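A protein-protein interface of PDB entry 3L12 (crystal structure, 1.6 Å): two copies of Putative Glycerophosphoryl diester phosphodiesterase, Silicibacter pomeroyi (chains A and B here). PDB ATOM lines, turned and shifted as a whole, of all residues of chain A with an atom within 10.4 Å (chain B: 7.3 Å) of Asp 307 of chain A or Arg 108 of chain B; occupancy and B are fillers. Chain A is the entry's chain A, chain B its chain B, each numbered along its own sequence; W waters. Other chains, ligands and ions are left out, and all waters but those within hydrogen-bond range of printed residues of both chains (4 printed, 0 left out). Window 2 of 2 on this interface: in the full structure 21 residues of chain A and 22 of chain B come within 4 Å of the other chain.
OD1 of Asp 307 of chain A is in salt-bridge range of NH1 of Arg 108 of chain B, at 3.6 Å.
The backbone carbonyl oxygen (O) of Gly 112 of chain B is in hydrogen-bond range of the guanidinium group (NH2) of Arg 303 of chain A, at 2.9 Å.
NH2 of Arg 283 of chain A lies within salt-bridge range of OD2 of Asp 307 of chain A (2.7 Å).
The side-chain carboxylate (OD1) of Asp 106 of chain B sits at hydrogen-bond distance from the backbone NH (N) of Arg 108 of chain B (3.0 Å).
The side-chain hydroxyl (OG1) of Thr 109 of chain B lies within hydrogen-bond range of the backbone NH (N) of Gly 112 of chain B (3.0 Å).
The backbone carbonyl oxygen (O) of Gly 107 of chain B lies within hydrogen-bond range of the guanidinium group (NE) of Arg 113 of chain B, at 2.9 Å.
Among the printed residues, merely in contact across the chains: Arg 303 of chain A with Leu 105 of chain B (3.8 Å) and Arg 303 of chain A with Gly 107 of chain B (3.8 Å).
Asp 307 of chain A touches just one residue of chain B: Arg 108 (3.0 Å).
Arg 108 of chain B touches one residue of chain A.
No residue of chain A comes within 4 Å of Asp 106 of chain B.
Of chain A, only Arg 303 (3.8 Å) comes within 4 Å of Gly 107 of chain B.
No residue of chain A comes within 4 Å of Thr 109 of chain B.
Of the printed residues of chain A, Leu 105 of chain B touches Arg 303.
Printed residues of chain B within 4 Å of Arg 303 of chain A: Leu 105, Gly 107 and Gly 112.
Of the printed residues of chain A, Gly 112 of chain B touches Arg 303 (2.9 Å).
Gly 299 of chain A touches none of the printed residues of chain B.
Ala 286 of chain A touches none of the printed residues of chain B.
The nearest residue of chain A that does not touch Arg 108 of chain B is Ile 306 of chain A (4.5 Å).
Along chain A the printed residues that touch a printed residue of chain B span positions 303 to 307.
Of the 10 printed residues of chain B, 4 touch a printed residue of chain A.
Among the printed residues, Asp or Glu carboxylates within 4 Å of a Lys or Arg side-chain nitrogen of the other chain: Asp 307 of chain A with Arg 108 of chain B (3.6 Å).
No position is printed for both chains.
Of the 4 pairs that touch across the chains among the printed residues, none has its exchanged pair printed and touching as well.
Water W3 lies within hydrogen-bond range of the side-chain carboxylate (OD1) of Asp 307 of chain A (2.6 Å), the guanidinium group (NH2) of Arg 113 of chain B (2.8 Å) and the backbone carbonyl oxygen (O) of Gly 107 of chain B (3.1 Å).
Water W1 bridges OD1 of Asp 307 of chain A (2.7 Å) and N of Gly 107 of chain B (3.3 Å).
Water W4 lies within hydrogen-bond range of O of Asp 307 of chain A, NH2 of Arg 108 of chain B and N of Gly 309 of chain A.
Water W2 bridges the guanidinium group of Arg 303 of chain A and the backbone NH of Leu 105 of chain B.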
ATOM      1  N   SER A  16       7.756  12.077  31.857  1.00  0.00           N
ATOM      2  CA  SER A  16       6.985  11.858  30.631  1.00  0.00           C
ATOM      3  C   SER A  16       6.779  13.078  29.770  1.00  0.00           C
ATOM      4  O   SER A  16       6.176  12.957  28.710  1.00  0.00           O
ATOM      5  CB  SER A  16       5.608  11.376  31.020  1.00  0.00           C
ATOM      6  OG  SER A  16       5.663  10.211  31.825  1.00  0.00           O
ATOM      7  N   PRO A 279      15.896  18.642  13.681  1.00  0.00           N
ATOM      8  CA  PRO A 279      15.455  17.416  14.337  1.00  0.00           C
ATOM      9  C   PRO A 279      16.450  16.749  15.270  1.00  0.00           C
ATOM     10  O   PRO A 279      16.076  16.327  16.391  1.00  0.00           O
ATOM     11  CB  PRO A 279      15.091  16.523  13.154  1.00  0.00           C
ATOM     12  CG  PRO A 279      14.879  17.396  12.049  1.00  0.00           C
ATOM     13  CD  PRO A 279      15.547  18.685  12.264  1.00  0.00           C
ATOM     14  N   ILE A 282      16.613  18.882  18.444  1.00  0.00           N
ATOM     15  CA  ILE A 282      15.380  18.695  19.272  1.00  0.00           C
ATOM     16  C   ILE A 282      15.481  17.407  20.053  1.00  0.00           C
ATOM     17  O   ILE A 282      15.320  17.374  21.285  1.00  0.00           O
ATOM     18  CB  ILE A 282      14.125  18.764  18.412  1.00  0.00           C
ATOM     19  CG1 ILE A 282      13.951  20.151  17.789  1.00  0.00           C
ATOM     20  CG2 ILE A 282      12.871  18.381  19.224  1.00  0.00           C
ATOM     21  CD1 ILE A 282      12.944  20.207  16.622  1.00  0.00           C
ATOM     22  N   ARG A 283      15.821  16.325  19.347  1.00  0.00           N
ATOM     23  CA  ARG A 283      16.004  15.029  19.967  1.00  0.00           C
ATOM     24  C   ARG A 283      17.075  15.044  21.057  1.00  0.00           C
ATOM     25  O   ARG A 283      16.849  14.522  22.136  1.00  0.00           O
ATOM     26  CB  ARG A 283      16.327  13.966  18.889  1.00  0.00           C
ATOM     27  CG  ARG A 283      16.437  12.570  19.394  1.00  0.00           C
ATOM     28  CD  ARG A 283      16.455  11.568  18.250  1.00  0.00           C
ATOM     29  NE  ARG A 283      15.197  11.502  17.526  1.00  0.00           N
ATOM     30  CZ  ARG A 283      14.180  10.682  17.837  1.00  0.00           C
ATOM     31  NH1 ARG A 283      14.274   9.796  18.808  1.00  0.00           N
ATOM     32  NH2 ARG A 283      13.085  10.712  17.102  1.00  0.00           N
ATOM     33  N   ALA A 286      15.792  16.939  24.167  1.00  0.00           N
ATOM     34  CA  ALA A 286      14.864  16.100  24.921  1.00  0.00           C
ATOM     35  C   ALA A 286      15.619  15.070  25.783  1.00  0.00           C
ATOM     36  O   ALA A 286      15.261  14.843  26.946  1.00  0.00           O
ATOM     37  CB  ALA A 286      13.808  15.418  23.986  1.00  0.00           C
ATOM     38  N   THR A 287      16.589  14.375  25.189  1.00  0.00           N
ATOM     39  CA  THR A 287      17.363  13.338  25.881  1.00  0.00           C
ATOM     40  C   THR A 287      18.140  13.858  27.096  1.00  0.00           C
ATOM     41  O   THR A 287      18.365  13.176  28.093  1.00  0.00           O
ATOM     42  CB  THR A 287      18.364  12.693  24.898  1.00  0.00           C
ATOM     43  OG1 THR A 287      17.641  12.129  23.799  1.00  0.00           O
ATOM     44  CG2 THR A 287      19.195  11.592  25.534  1.00  0.00           C
ATOM     45  N   GLY A 299       5.189  22.075  15.555  1.00  0.00           N
ATOM     46  CA  GLY A 299       4.717  20.777  15.088  1.00  0.00           C
ATOM     47  C   GLY A 299       5.854  19.786  14.971  1.00  0.00           C
ATOM     48  O   GLY A 299       5.688  18.625  15.313  1.00  0.00           O
ATOM     49  N   ARG A 300       6.987  20.209  14.387  1.00  0.00           N
ATOM     50  CA  ARG A 300       8.175  19.373  14.255  1.00  0.00           C
ATOM     51  C   ARG A 300       8.598  18.839  15.607  1.00  0.00           C
ATOM     52  O   ARG A 300       8.940  17.641  15.742  1.00  0.00           O
ATOM     53  CB  ARG A 300       9.277  20.208  13.615  1.00  0.00           C
ATOM     54  CG  ARG A 300      10.574  19.435  13.462  1.00  0.00           C
ATOM     55  CD  ARG A 300      11.680  20.335  12.895  1.00  0.00           C
ATOM     56  NE  ARG A 300      11.292  20.806  11.550  1.00  0.00           N
ATOM     57  CZ  ARG A 300      11.954  21.752  10.882  1.00  0.00           C
ATOM     58  NH1 ARG A 300      12.995  22.399  11.435  1.00  0.00           N
ATOM     59  NH2 ARG A 300      11.579  22.070   9.655  1.00  0.00           N
ATOM     60  N   THR A 301       8.603  19.745  16.602  1.00  0.00           N
ATOM     61  CA  THR A 301       8.993  19.410  17.974  1.00  0.00           C
ATOM     62  C   THR A 301       8.007  18.440  18.594  1.00  0.00           C
ATOM     63  O   THR A 301       8.380  17.432  19.224  1.00  0.00           O
ATOM     64  CB  THR A 301       9.161  20.685  18.797  1.00  0.00           C
ATOM     65  OG1 THR A 301      10.194  21.486  18.193  1.00  0.00           O
ATOM     66  CG2 THR A 301       9.599  20.312  20.232  1.00  0.00           C
ATOM     67  N   GLN A 302       6.723  18.721  18.460  1.00  0.00           N
ATOM     68  CA  GLN A 302       5.685  17.795  18.943  1.00  0.00           C
ATOM     69  C   GLN A 302       5.886  16.398  18.383  1.00  0.00           C
ATOM     70  O   GLN A 302       5.824  15.406  19.118  1.00  0.00           O
ATOM     71  CB  GLN A 302       4.319  18.273  18.520  1.00  0.00           C
ATOM     72  CG  GLN A 302       3.786  19.517  19.231  1.00  0.00           C
ATOM     73  CD  GLN A 302       2.556  20.135  18.584  1.00  0.00           C
ATOM     74  OE1 GLN A 302       2.122  19.766  17.460  1.00  0.00           O
ATOM     75  NE2 GLN A 302       1.987  21.108  19.272  1.00  0.00           N
ATOM     76  N   ARG A 303       6.100  16.303  17.062  1.00  0.00           N
ATOM     77  CA  ARG A 303       6.256  14.986  16.432  1.00  0.00           C
ATOM     78  C   ARG A 303       7.469  14.190  16.926  1.00  0.00           C
ATOM     79  O   ARG A 303       7.393  12.970  17.106  1.00  0.00           O
ATOM     80  CB  ARG A 303       6.229  15.153  14.924  1.00  0.00           C
ATOM     81  CG  ARG A 303       4.837  15.439  14.422  1.00  0.00           C
ATOM     82  CD  ARG A 303       3.910  14.163  14.375  1.00  0.00           C
ATOM     83  NE  ARG A 303       4.529  13.219  13.449  1.00  0.00           N
ATOM     84  CZ  ARG A 303       4.442  13.289  12.132  1.00  0.00           C
ATOM     85  NH1 ARG A 303       3.526  14.064  11.538  1.00  0.00           N
ATOM     86  NH2 ARG A 303       5.237  12.529  11.405  1.00  0.00           N
ATOM     87  N   ILE A 304       8.532  14.893  17.206  1.00  0.00           N
ATOM     88  CA  ILE A 304       9.747  14.255  17.760  1.00  0.00           C
ATOM     89  C   ILE A 304       9.469  13.793  19.188  1.00  0.00           C
ATOM     90  O   ILE A 304       9.773  12.665  19.524  1.00  0.00           O
ATOM     91  CB  ILE A 304      10.981  15.156  17.668  1.00  0.00           C
ATOM     92  CG1 ILE A 304      11.470  15.224  16.208  1.00  0.00           C
ATOM     93  CG2 ILE A 304      12.066  14.662  18.589  1.00  0.00           C
ATOM     94  CD1 ILE A 304      12.367  16.365  15.945  1.00  0.00           C
ATOM     95  N   LEU A 305       8.768  14.609  19.982  1.00  0.00           N
ATOM     96  CA  LEU A 305       8.416  14.173  21.349  1.00  0.00           C
ATOM     97  C   LEU A 305       7.506  12.950  21.322  1.00  0.00           C
ATOM     98  O   LEU A 305       7.754  11.968  22.015  1.00  0.00           O
ATOM     99  CB  LEU A 305       7.840  15.306  22.194  1.00  0.00           C
ATOM    100  CG  LEU A 305       8.771  16.496  22.460  1.00  0.00           C
ATOM    101  CD1 LEU A 305       8.045  17.646  23.159  1.00  0.00           C
ATOM    102  CD2 LEU A 305      10.003  16.068  23.282  1.00  0.00           C
ATOM    103  N   ILE A 306       6.499  12.962  20.455  1.00  0.00           N
ATOM    104  CA  ILE A 306       5.639  11.790  20.320  1.00  0.00           C
ATOM    105  C   ILE A 306       6.433  10.544  19.875  1.00  0.00           C
ATOM    106  O   ILE A 306       6.225   9.462  20.379  1.00  0.00           O
ATOM    107  CB  ILE A 306       4.479  12.051  19.295  1.00  0.00           C
ATOM    108  CG1 ILE A 306       3.470  13.090  19.801  1.00  0.00           C
ATOM    109  CG2 ILE A 306       3.788  10.747  18.886  1.00  0.00           C
ATOM    110  CD1 ILE A 306       2.811  12.774  21.117  1.00  0.00           C
ATOM    111  N   ASP A 307       7.349  10.712  18.929  1.00  0.00           N
ATOM    112  CA  ASP A 307       8.185   9.618  18.479  1.00  0.00           C
ATOM    113  C   ASP A 307       9.041   9.021  19.641  1.00  0.00           C
ATOM    114  O   ASP A 307       9.341   7.811  19.677  1.00  0.00           O
ATOM    115  CB  ASP A 307       9.124  10.086  17.380  1.00  0.00           C
ATOM    116  CG  ASP A 307       9.955   8.929  16.851  1.00  0.00           C
ATOM    117  OD1 ASP A 307       9.376   8.099  16.102  1.00  0.00           O
ATOM    118  OD2 ASP A 307      11.143   8.794  17.285  1.00  0.00           O
ATOM    119  N   MET A 308       9.388   9.879  20.585  1.00  0.00           N
ATOM    120  CA  MET A 308      10.133   9.501  21.805  1.00  0.00           C
ATOM    121  C   MET A 308       9.248   9.052  22.948  1.00  0.00           C
ATOM    122  O   MET A 308       9.734   8.774  24.046  1.00  0.00           O
ATOM    123  CB  MET A 308      11.016  10.707  22.306  1.00  0.00           C
ATOM    124  CG  MET A 308      12.009  11.096  21.267  1.00  0.00           C
ATOM    125  SD  MET A 308      13.044  12.649  21.733  1.00  0.00           S
ATOM    126  CE  MET A 308      14.164  11.948  23.147  1.00  0.00           C
ATOM    127  N   GLY A 309       7.954   8.907  22.707  1.00  0.00           N
ATOM    128  CA  GLY A 309       7.025   8.479  23.733  1.00  0.00           C
ATOM    129  C   GLY A 309       6.687   9.494  24.796  1.00  0.00           C
ATOM    130  O   GLY A 309       6.137   9.112  25.839  1.00  0.00           O
ATOM    131  N   LEU A 310       7.017  10.759  24.545  1.00  0.00           N
ATOM    132  CA  LEU A 310       6.824  11.844  25.496  1.00  0.00           C
ATOM    133  C   LEU A 310       5.598  12.673  25.076  1.00  0.00           C
ATOM    134  O   LEU A 310       4.999  12.453  24.030  1.00  0.00           O
ATOM    135  CB  LEU A 310       8.070  12.717  25.541  1.00  0.00           C
ATOM    136  CG  LEU A 310       9.391  12.003  25.930  1.00  0.00           C
ATOM    137  CD1 LEU A 310      10.640  12.841  25.654  1.00  0.00           C
ATOM    138  CD2 LEU A 310       9.338  11.526  27.373  1.00  0.00           C
ATOM    139  N   SER A 311       5.255  13.655  25.905  1.00  0.00           N
ATOM    140  CA  SER A 311       4.191  14.576  25.580  1.00  0.00           C
ATOM    141  C   SER A 311       4.572  15.930  26.166  1.00  0.00           C
ATOM    142  O   SER A 311       5.595  16.064  26.839  1.00  0.00           O
ATOM    143  CB  SER A 311       2.889  14.054  26.165  1.00  0.00           C
ATOM    144  OG  SER A 311       2.932  14.050  27.578  1.00  0.00           O
ATOM    145  N   TRP A 312       3.734  16.916  25.948  1.00  0.00           N
ATOM    146  CA  TRP A 312       4.038  18.323  26.387  1.00  0.00           C
ATOM    147  C   TRP A 312       3.009  18.904  27.293  1.00  0.00           C
ATOM    148  O   TRP A 312       3.209  19.998  27.801  1.00  0.00           O
ATOM    149  CB  TRP A 312       4.300  19.245  25.189  1.00  0.00           C
ATOM    150  CG  TRP A 312       3.205  19.171  24.229  1.00  0.00           C
ATOM    151  CD1 TRP A 312       2.064  19.912  24.221  1.00  0.00           C
ATOM    152  CD2 TRP A 312       3.078  18.229  23.141  1.00  0.00           C
ATOM    153  NE1 TRP A 312       1.254  19.509  23.174  1.00  0.00           N
ATOM    154  CE2 TRP A 312       1.852  18.465  22.518  1.00  0.00           C
ATOM    155  CE3 TRP A 312       3.869  17.208  22.663  1.00  0.00           C
ATOM    156  CZ2 TRP A 312       1.425  17.690  21.409  1.00  0.00           C
ATOM    157  CZ3 TRP A 312       3.456  16.458  21.617  1.00  0.00           C
ATOM    158  CH2 TRP A 312       2.245  16.702  20.990  1.00  0.00           C
ATOM    159  N   TRP B  81      -3.036   4.029  17.962  1.00  0.00           N
ATOM    160  CA  TRP B  81      -3.157   3.886  16.512  1.00  0.00           C
ATOM    161  C   TRP B  81      -3.988   2.641  16.243  1.00  0.00           C
ATOM    162  O   TRP B  81      -3.817   1.581  16.904  1.00  0.00           O
ATOM    163  CB  TRP B  81      -1.788   3.739  15.815  1.00  0.00           C
ATOM    164  CG  TRP B  81      -0.959   4.925  16.063  1.00  0.00           C
ATOM    165  CD1 TRP B  81       0.187   5.006  16.846  1.00  0.00           C
ATOM    166  CD2 TRP B  81      -1.165   6.211  15.505  1.00  0.00           C
ATOM    167  NE1 TRP B  81       0.668   6.309  16.811  1.00  0.00           N
ATOM    168  CE2 TRP B  81      -0.186   7.074  16.052  1.00  0.00           C
ATOM    169  CE3 TRP B  81      -2.112   6.743  14.624  1.00  0.00           C
ATOM    170  CZ2 TRP B  81      -0.134   8.420  15.714  1.00  0.00           C
ATOM    171  CZ3 TRP B  81      -2.080   8.081  14.321  1.00  0.00           C
ATOM    172  CH2 TRP B  81      -1.099   8.919  14.876  1.00  0.00           C
ATOM    173  N   LEU B 105      -0.352  12.114  12.655  1.00  0.00           N
ATOM    174  CA  LEU B 105       0.156  11.004  11.942  1.00  0.00           C
ATOM    175  C   LEU B 105       1.139  10.203  12.806  1.00  0.00           C
ATOM    176  O   LEU B 105       1.735  10.706  13.755  1.00  0.00           O
ATOM    177  CB  LEU B 105       0.928  11.480  10.696  1.00  0.00           C
ATOM    178  CG  LEU B 105       0.157  12.263   9.655  1.00  0.00           C
ATOM    179  CD1 LEU B 105       1.144  12.750   8.578  1.00  0.00           C
ATOM    180  CD2 LEU B 105      -0.911  11.356   9.132  1.00  0.00           C
ATOM    181  N   ASP B 106       1.233   8.930  12.463  1.00  0.00           N
ATOM    182  CA  ASP B 106       2.150   8.008  13.101  1.00  0.00           C
ATOM    183  C   ASP B 106       3.511   8.170  12.455  1.00  0.00           C
ATOM    184  O   ASP B 106       3.713   7.716  11.300  1.00  0.00           O
ATOM    185  CB  ASP B 106       1.636   6.577  12.961  1.00  0.00           C
ATOM    186  CG  ASP B 106       2.472   5.575  13.704  1.00  0.00           C
ATOM    187  OD1 ASP B 106       3.655   5.869  14.102  1.00  0.00           O
ATOM    188  OD2 ASP B 106       2.024   4.415  13.871  1.00  0.00           O
ATOM    189  N   GLY B 107       4.479   8.754  13.192  1.00  0.00           N
ATOM    190  CA  GLY B 107       5.785   9.019  12.656  1.00  0.00           C
ATOM    191  C   GLY B 107       6.689   7.810  12.380  1.00  0.00           C
ATOM    192  O   GLY B 107       7.800   7.963  11.875  1.00  0.00           O
ATOM    193  N   ARG B 108       6.244   6.616  12.756  1.00  0.00           N
ATOM    194  CA  ARG B 108       6.948   5.374  12.484  1.00  0.00           C
ATOM    195  C   ARG B 108       6.502   4.765  11.140  1.00  0.00           C
ATOM    196  O   ARG B 108       7.102   3.764  10.691  1.00  0.00           O
ATOM    197  CB  ARG B 108       6.728   4.411  13.632  1.00  0.00           C
ATOM    198  CG  ARG B 108       7.563   4.782  14.875  1.00  0.00           C
ATOM    199  CD  ARG B 108       7.276   3.778  16.012  1.00  0.00           C
ATOM    200  NE  ARG B 108       8.279   3.918  17.076  1.00  0.00           N
ATOM    201  CZ  ARG B 108       8.296   4.900  17.969  1.00  0.00           C
ATOM    202  NH1 ARG B 108       7.338   5.805  18.023  1.00  0.00           N
ATOM    203  NH2 ARG B 108       9.252   4.940  18.863  1.00  0.00           N
ATOM    204  N   THR B 109       5.538   5.397  10.472  1.00  0.00           N
ATOM    205  CA  THR B 109       5.005   4.880   9.200  1.00  0.00           C
ATOM    206  C   THR B 109       5.599   5.659   8.036  1.00  0.00           C
ATOM    207  O   THR B 109       6.071   6.794   8.179  1.00  0.00           O
ATOM    208  CB  THR B 109       3.468   4.952   9.135  1.00  0.00           C
ATOM    209  OG1 THR B 109       3.024   6.331   9.081  1.00  0.00           O
ATOM    210  CG2 THR B 109       2.862   4.193  10.315  1.00  0.00           C
ATOM    211  N   VAL B 110       5.617   5.033   6.858  1.00  0.00           N
ATOM    212  CA  VAL B 110       6.053   5.725   5.668  1.00  0.00           C
ATOM    213  C   VAL B 110       5.232   7.033   5.403  1.00  0.00           C
ATOM    214  O   VAL B 110       5.783   8.096   5.171  1.00  0.00           O
ATOM    215  CB  VAL B 110       5.909   4.791   4.422  1.00  0.00           C
ATOM    216  CG1 VAL B 110       6.210   5.641   3.144  1.00  0.00           C
ATOM    217  CG2 VAL B 110       6.803   3.553   4.545  1.00  0.00           C
ATOM    218  N   TYR B 111       3.910   6.971   5.517  1.00  0.00           N
ATOM    219  CA  TYR B 111       3.078   8.155   5.278  1.00  0.00           C
ATOM    220  C   TYR B 111       3.389   9.229   6.291  1.00  0.00           C
ATOM    221  O   TYR B 111       3.543  10.377   5.944  1.00  0.00           O
ATOM    222  CB  TYR B 111       1.603   7.783   5.343  1.00  0.00           C
ATOM    223  CG  TYR B 111       0.679   8.862   4.884  1.00  0.00           C
ATOM    224  CD1 TYR B 111       0.481   9.088   3.517  1.00  0.00           C
ATOM    225  CD2 TYR B 111      -0.009   9.665   5.772  1.00  0.00           C
ATOM    226  CE1 TYR B 111      -0.307  10.098   3.062  1.00  0.00           C
ATOM    227  CE2 TYR B 111      -0.871  10.667   5.323  1.00  0.00           C
ATOM    228  CZ  TYR B 111      -1.032  10.878   3.949  1.00  0.00           C
ATOM    229  OH  TYR B 111      -1.933  11.837   3.523  1.00  0.00           O
ATOM    230  N   GLY B 112       3.475   8.847   7.578  1.00  0.00           N
ATOM    231  CA  GLY B 112       3.774   9.825   8.617  1.00  0.00           C
ATOM    232  C   GLY B 112       5.127  10.506   8.393  1.00  0.00           C
ATOM    233  O   GLY B 112       5.277  11.720   8.632  1.00  0.00           O
ATOM    234  N   ARG B 113       6.135   9.747   7.922  1.00  0.00           N
ATOM    235  CA  ARG B 113       7.458  10.292   7.679  1.00  0.00           C
ATOM    236  C   ARG B 113       7.528  11.282   6.503  1.00  0.00           C
ATOM    237  O   ARG B 113       8.507  12.035   6.397  1.00  0.00           O
ATOM    238  CB  ARG B 113       8.530   9.197   7.572  1.00  0.00           C
ATOM    239  CG  ARG B 113       8.744   8.489   8.893  1.00  0.00           C
ATOM    240  CD  ARG B 113       9.536   7.209   8.815  1.00  0.00           C
ATOM    241  NE  ARG B 113       9.849   6.807  10.198  1.00  0.00           N
ATOM    242  CZ  ARG B 113      10.598   5.767  10.547  1.00  0.00           C
ATOM    243  NH1 ARG B 113      11.154   5.011   9.606  1.00  0.00           N
ATOM    244  NH2 ARG B 113      10.866   5.523  11.849  1.00  0.00           N
HETATM  245  O   HOH W   1       6.866   8.811  15.517  1.00  0.00           O
HETATM  246  O   HOH W   2       0.867  14.902  12.691  1.00  0.00           O
HETATM  247  O   HOH W   3      10.199   7.539  13.729  1.00  0.00           O
HETATM  248  O   HOH W   4       9.696   6.042  21.740  1.00  0.00           O
